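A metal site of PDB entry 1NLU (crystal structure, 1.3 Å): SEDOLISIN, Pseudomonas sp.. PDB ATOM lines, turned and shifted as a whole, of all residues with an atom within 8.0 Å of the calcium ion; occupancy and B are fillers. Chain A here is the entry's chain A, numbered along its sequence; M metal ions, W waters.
OD1 of Asp 348 sits at hydrogen-bond distance from OG1 of Thr 351 (2.7 Å).
The side-chain carboxylate (OD2) of Asp 328 is in salt-bridge range of the side-chain amino group (NZ) of Lys 330 (3.5 Å).
Of the 20 residues printed, 5 come within 4 Å of the calcium ion.
Along chain A the residues within 4 Å of the calcium ion span positions 328 to 348.
The calcium ion is bound by OD1 of Asp 328 (2.3 Å), O of Val 329 (2.4 Å), O of Gly 346 (2.4 Å), OD2 of Asp 348 (2.4 Å), O of Gly 344 (2.4 Å) and water W1 (2.4 Å).
The calcium ion has six donor atoms within binding distance.
Water W1 lies within hydrogen-bond range of O of Gly 352, OG1 of Thr 351, N of Gly 354 and N of Val 329.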
ATOM      1  N   VAL A 219       4.745  -4.755  25.607  1.00  0.00           N
ATOM      2  CA  VAL A 219       3.980  -5.788  24.953  1.00  0.00           C
ATOM      3  C   VAL A 219       4.871  -6.989  24.643  1.00  0.00           C
ATOM      4  O   VAL A 219       6.042  -6.828  24.240  1.00  0.00           O
ATOM      5  CB  VAL A 219       3.426  -5.222  23.635  1.00  0.00           C
ATOM      6  CG1 VAL A 219       2.709  -6.267  22.813  1.00  0.00           C
ATOM      7  CG2 VAL A 219       2.521  -4.014  23.913  1.00  0.00           C
ATOM      8  N   VAL A 326      -2.931  -1.481  38.635  1.00  0.00           N
ATOM      9  CA  VAL A 326      -2.271  -2.216  37.540  1.00  0.00           C
ATOM     10  C   VAL A 326      -0.897  -1.628  37.227  1.00  0.00           C
ATOM     11  O   VAL A 326      -0.642  -0.472  37.558  1.00  0.00           O
ATOM     12  CB  VAL A 326      -3.132  -2.287  36.259  1.00  0.00           C
ATOM     13  CG1 VAL A 326      -4.358  -3.162  36.518  1.00  0.00           C
ATOM     14  CG2 VAL A 326      -3.554  -0.906  35.761  1.00  0.00           C
ATOM     15  N   HIS A 327      -0.106  -2.450  36.561  1.00  0.00           N
ATOM     16  CA  HIS A 327       1.021  -1.959  35.787  1.00  0.00           C
ATOM     17  C   HIS A 327       0.539  -1.722  34.348  1.00  0.00           C
ATOM     18  O   HIS A 327       0.273  -2.692  33.657  1.00  0.00           O
ATOM     19  CB  HIS A 327       2.193  -2.907  35.808  1.00  0.00           C
ATOM     20  CG  HIS A 327       2.738  -3.202  37.147  1.00  0.00           C
ATOM     21  ND1 HIS A 327       3.443  -2.244  37.856  1.00  0.00           N
ATOM     22  CD2 HIS A 327       2.732  -4.297  37.916  1.00  0.00           C
ATOM     23  CE1 HIS A 327       3.843  -2.757  39.018  1.00  0.00           C
ATOM     24  NE2 HIS A 327       3.412  -3.999  39.079  1.00  0.00           N
ATOM     25  N   ASP A 328       0.405  -0.454  33.962  1.00  0.00           N
ATOM     26  CA  ASP A 328      -0.124  -0.125  32.642  1.00  0.00           C
ATOM     27  C   ASP A 328       0.955  -0.313  31.596  1.00  0.00           C
ATOM     28  O   ASP A 328       1.983   0.367  31.570  1.00  0.00           O
ATOM     29  CB  ASP A 328      -0.585   1.336  32.687  1.00  0.00           C
ATOM     30  CG  ASP A 328      -1.208   1.803  31.411  1.00  0.00           C
ATOM     31  OD1 ASP A 328      -1.577   0.918  30.577  1.00  0.00           O
ATOM     32  OD2 ASP A 328      -1.369   3.004  31.179  1.00  0.00           O
ATOM     33  N   VAL A 329       0.845  -1.227  30.674  1.00  0.00           N
ATOM     34  CA  VAL A 329       1.811  -1.406  29.592  1.00  0.00           C
ATOM     35  C   VAL A 329       1.589  -0.311  28.573  1.00  0.00           C
ATOM     36  O   VAL A 329       0.420  -0.105  28.154  1.00  0.00           O
ATOM     37  CB  VAL A 329       1.633  -2.782  28.947  1.00  0.00           C
ATOM     38  CG1 VAL A 329       2.553  -2.908  27.749  1.00  0.00           C
ATOM     39  CG2 VAL A 329       1.882  -3.889  29.999  1.00  0.00           C
ATOM     40  N   LYS A 330       2.607   0.399  28.107  1.00  0.00           N
ATOM     41  CA  LYS A 330       2.438   1.530  27.228  1.00  0.00           C
ATOM     42  C   LYS A 330       3.253   1.403  25.944  1.00  0.00           C
ATOM     43  O   LYS A 330       2.982   2.161  25.018  1.00  0.00           O
ATOM     44  CB  LYS A 330       2.795   2.831  27.942  1.00  0.00           C
ATOM     45  CG  LYS A 330       1.827   3.167  29.070  1.00  0.00           C
ATOM     46  CD  LYS A 330       2.390   4.360  29.875  1.00  0.00           C
ATOM     47  CE  LYS A 330       1.763   4.229  31.250  1.00  0.00           C
ATOM     48  NZ  LYS A 330       1.059   5.480  31.648  1.00  0.00           N
ATOM     49  N   SER A 331       4.216   0.461  25.856  1.00  0.00           N
ATOM     50  CA  SER A 331       5.104   0.396  24.729  1.00  0.00           C
ATOM     51  C   SER A 331       4.994  -0.932  23.994  1.00  0.00           C
ATOM     52  O   SER A 331       5.068  -1.957  24.686  1.00  0.00           O
ATOM     53  CB  SER A 331       6.560   0.543  25.224  1.00  0.00           C
ATOM     54  OG  SER A 331       7.463   0.282  24.181  1.00  0.00           O
ATOM     55  N   ASN A 342      -1.313  -1.033  18.833  1.00  0.00           N
ATOM     56  CA  ASN A 342      -0.268  -0.443  19.692  1.00  0.00           C
ATOM     57  C   ASN A 342      -0.727  -0.343  21.130  1.00  0.00           C
ATOM     58  O   ASN A 342      -1.882  -0.023  21.428  1.00  0.00           O
ATOM     59  CB  ASN A 342       0.038   0.977  19.191  1.00  0.00           C
ATOM     60  CG  ASN A 342       0.563   0.945  17.752  1.00  0.00           C
ATOM     61  OD1 ASN A 342       1.550   0.270  17.486  1.00  0.00           O
ATOM     62  ND2 ASN A 342      -0.113   1.699  16.885  1.00  0.00           N
ATOM     63  N   ALA A 343       0.169  -0.590  22.086  1.00  0.00           N
ATOM     64  CA  ALA A 343      -0.094  -0.306  23.479  1.00  0.00           C
ATOM     65  C   ALA A 343      -0.164   1.210  23.692  1.00  0.00           C
ATOM     66  O   ALA A 343       0.342   2.018  22.901  1.00  0.00           O
ATOM     67  CB  ALA A 343       0.980  -0.895  24.379  1.00  0.00           C
ATOM     68  N   GLY A 344      -0.820   1.621  24.770  1.00  0.00           N
ATOM     69  CA  GLY A 344      -0.844   3.053  25.061  1.00  0.00           C
ATOM     70  C   GLY A 344      -1.382   3.244  26.477  1.00  0.00           C
ATOM     71  O   GLY A 344      -1.518   2.292  27.264  1.00  0.00           O
ATOM     72  N   THR A 345      -1.698   4.452  26.881  1.00  0.00           N
ATOM     73  CA  THR A 345      -2.202   4.718  28.215  1.00  0.00           C
ATOM     74  C   THR A 345      -3.524   4.023  28.448  1.00  0.00           C
ATOM     75  O   THR A 345      -4.416   4.104  27.579  1.00  0.00           O
ATOM     76  CB  THR A 345      -2.397   6.239  28.332  1.00  0.00           C
ATOM     77  OG1 THR A 345      -1.082   6.816  28.310  1.00  0.00           O
ATOM     78  CG2 THR A 345      -3.018   6.628  29.665  1.00  0.00           C
ATOM     79  N   GLY A 346      -3.673   3.352  29.591  1.00  0.00           N
ATOM     80  CA  GLY A 346      -4.913   2.676  29.925  1.00  0.00           C
ATOM     81  C   GLY A 346      -5.139   1.409  29.112  1.00  0.00           C
ATOM     82  O   GLY A 346      -4.203   0.762  28.671  1.00  0.00           O
ATOM     83  N   TRP A 347      -6.405   1.016  28.929  1.00  0.00           N
ATOM     84  CA  TRP A 347      -6.682  -0.262  28.250  1.00  0.00           C
ATOM     85  C   TRP A 347      -6.200  -0.179  26.828  1.00  0.00           C
ATOM     86  O   TRP A 347      -6.470   0.830  26.176  1.00  0.00           O
ATOM     87  CB  TRP A 347      -8.183  -0.516  28.339  1.00  0.00           C
ATOM     88  CG  TRP A 347      -8.552  -1.939  27.923  1.00  0.00           C
ATOM     89  CD1 TRP A 347      -8.823  -2.968  28.796  1.00  0.00           C
ATOM     90  CD2 TRP A 347      -8.690  -2.446  26.603  1.00  0.00           C
ATOM     91  NE1 TRP A 347      -9.119  -4.081  28.073  1.00  0.00           N
ATOM     92  CE2 TRP A 347      -9.039  -3.810  26.706  1.00  0.00           C
ATOM     93  CE3 TRP A 347      -8.539  -1.898  25.308  1.00  0.00           C
ATOM     94  CZ2 TRP A 347      -9.249  -4.647  25.605  1.00  0.00           C
ATOM     95  CZ3 TRP A 347      -8.747  -2.731  24.197  1.00  0.00           C
ATOM     96  CH2 TRP A 347      -9.086  -4.078  24.356  1.00  0.00           C
ATOM     97  N   ASP A 348      -5.571  -1.228  26.317  1.00  0.00           N
ATOM     98  CA  ASP A 348      -5.211  -1.273  24.891  1.00  0.00           C
ATOM     99  C   ASP A 348      -5.393  -2.692  24.370  1.00  0.00           C
ATOM    100  O   ASP A 348      -5.574  -3.675  25.123  1.00  0.00           O
ATOM    101  CB  ASP A 348      -3.810  -0.728  24.707  1.00  0.00           C
ATOM    102  CG  ASP A 348      -2.764  -1.501  25.476  1.00  0.00           C
ATOM    103  OD1 ASP A 348      -2.599  -2.709  25.400  1.00  0.00           O
ATOM    104  OD2 ASP A 348      -2.043  -0.789  26.221  1.00  0.00           O
ATOM    105  N   TYR A 349      -5.409  -2.846  23.056  1.00  0.00           N
ATOM    106  CA  TYR A 349      -5.705  -4.165  22.478  1.00  0.00           C
ATOM    107  C   TYR A 349      -4.583  -5.169  22.711  1.00  0.00           C
ATOM    108  O   TYR A 349      -4.915  -6.363  22.824  1.00  0.00           O
ATOM    109  CB  TYR A 349      -6.011  -4.017  20.999  1.00  0.00           C
ATOM    110  CG  TYR A 349      -7.372  -3.416  20.693  1.00  0.00           C
ATOM    111  CD1 TYR A 349      -7.504  -2.129  20.181  1.00  0.00           C
ATOM    112  CD2 TYR A 349      -8.527  -4.175  20.954  1.00  0.00           C
ATOM    113  CE1 TYR A 349      -8.798  -1.653  19.936  1.00  0.00           C
ATOM    114  CE2 TYR A 349      -9.803  -3.708  20.696  1.00  0.00           C
ATOM    115  CZ  TYR A 349      -9.921  -2.422  20.174  1.00  0.00           C
ATOM    116  OH  TYR A 349     -11.172  -1.896  19.916  1.00  0.00           O
ATOM    117  N   PRO A 350      -3.302  -4.830  22.733  1.00  0.00           N
ATOM    118  CA  PRO A 350      -2.339  -5.910  22.994  1.00  0.00           C
ATOM    119  C   PRO A 350      -2.416  -6.474  24.382  1.00  0.00           C
ATOM    120  O   PRO A 350      -2.175  -7.681  24.579  1.00  0.00           O
ATOM    121  CB  PRO A 350      -0.961  -5.245  22.754  1.00  0.00           C
ATOM    122  CG  PRO A 350      -1.297  -4.167  21.731  1.00  0.00           C
ATOM    123  CD  PRO A 350      -2.624  -3.588  22.257  1.00  0.00           C
ATOM    124  N   THR A 351      -2.689  -5.662  25.396  1.00  0.00           N
ATOM    125  CA  THR A 351      -2.480  -6.091  26.785  1.00  0.00           C
ATOM    126  C   THR A 351      -3.663  -5.824  27.696  1.00  0.00           C
ATOM    127  O   THR A 351      -3.564  -6.160  28.888  1.00  0.00           O
ATOM    128  CB  THR A 351      -1.214  -5.435  27.406  1.00  0.00           C
ATOM    129  OG1 THR A 351      -1.334  -3.997  27.413  1.00  0.00           O
ATOM    130  CG2 THR A 351       0.027  -5.854  26.608  1.00  0.00           C
ATOM    131  N   GLY A 352      -4.759  -5.247  27.216  1.00  0.00           N
ATOM    132  CA  GLY A 352      -5.871  -4.915  28.082  1.00  0.00           C
ATOM    133  C   GLY A 352      -5.437  -3.917  29.142  1.00  0.00           C
ATOM    134  O   GLY A 352      -4.803  -2.924  28.782  1.00  0.00           O
ATOM    135  N   TRP A 353      -5.784  -4.156  30.415  1.00  0.00           N
ATOM    136  CA  TRP A 353      -5.412  -3.212  31.449  1.00  0.00           C
ATOM    137  C   TRP A 353      -3.960  -3.366  31.893  1.00  0.00           C
ATOM    138  O   TRP A 353      -3.510  -2.563  32.733  1.00  0.00           O
ATOM    139  CB  TRP A 353      -6.322  -3.453  32.656  1.00  0.00           C
ATOM    140  CG  TRP A 353      -7.754  -3.062  32.481  1.00  0.00           C
ATOM    141  CD1 TRP A 353      -8.827  -3.863  32.463  1.00  0.00           C
ATOM    142  CD2 TRP A 353      -8.241  -1.708  32.276  1.00  0.00           C
ATOM    143  NE1 TRP A 353      -9.977  -3.117  32.275  1.00  0.00           N
ATOM    144  CE2 TRP A 353      -9.644  -1.792  32.161  1.00  0.00           C
ATOM    145  CE3 TRP A 353      -7.600  -0.457  32.206  1.00  0.00           C
ATOM    146  CZ2 TRP A 353     -10.452  -0.660  31.951  1.00  0.00           C
ATOM    147  CZ3 TRP A 353      -8.384   0.660  32.004  1.00  0.00           C
ATOM    148  CH2 TRP A 353      -9.806   0.566  31.891  1.00  0.00           C
ATOM    149  N   GLY A 354      -3.257  -4.386  31.397  1.00  0.00           N
ATOM    150  CA  GLY A 354      -1.901  -4.653  31.916  1.00  0.00           C
ATOM    151  C   GLY A 354      -1.931  -5.668  33.050  1.00  0.00           C
ATOM    152  O   GLY A 354      -2.896  -6.429  33.169  1.00  0.00           O
HETATM  153 CA    CA M   1      -1.915   0.222  28.372  1.00  0.00          CA
HETATM  154  O   HOH W   1      -2.208  -2.050  29.236  1.00  0.00           O
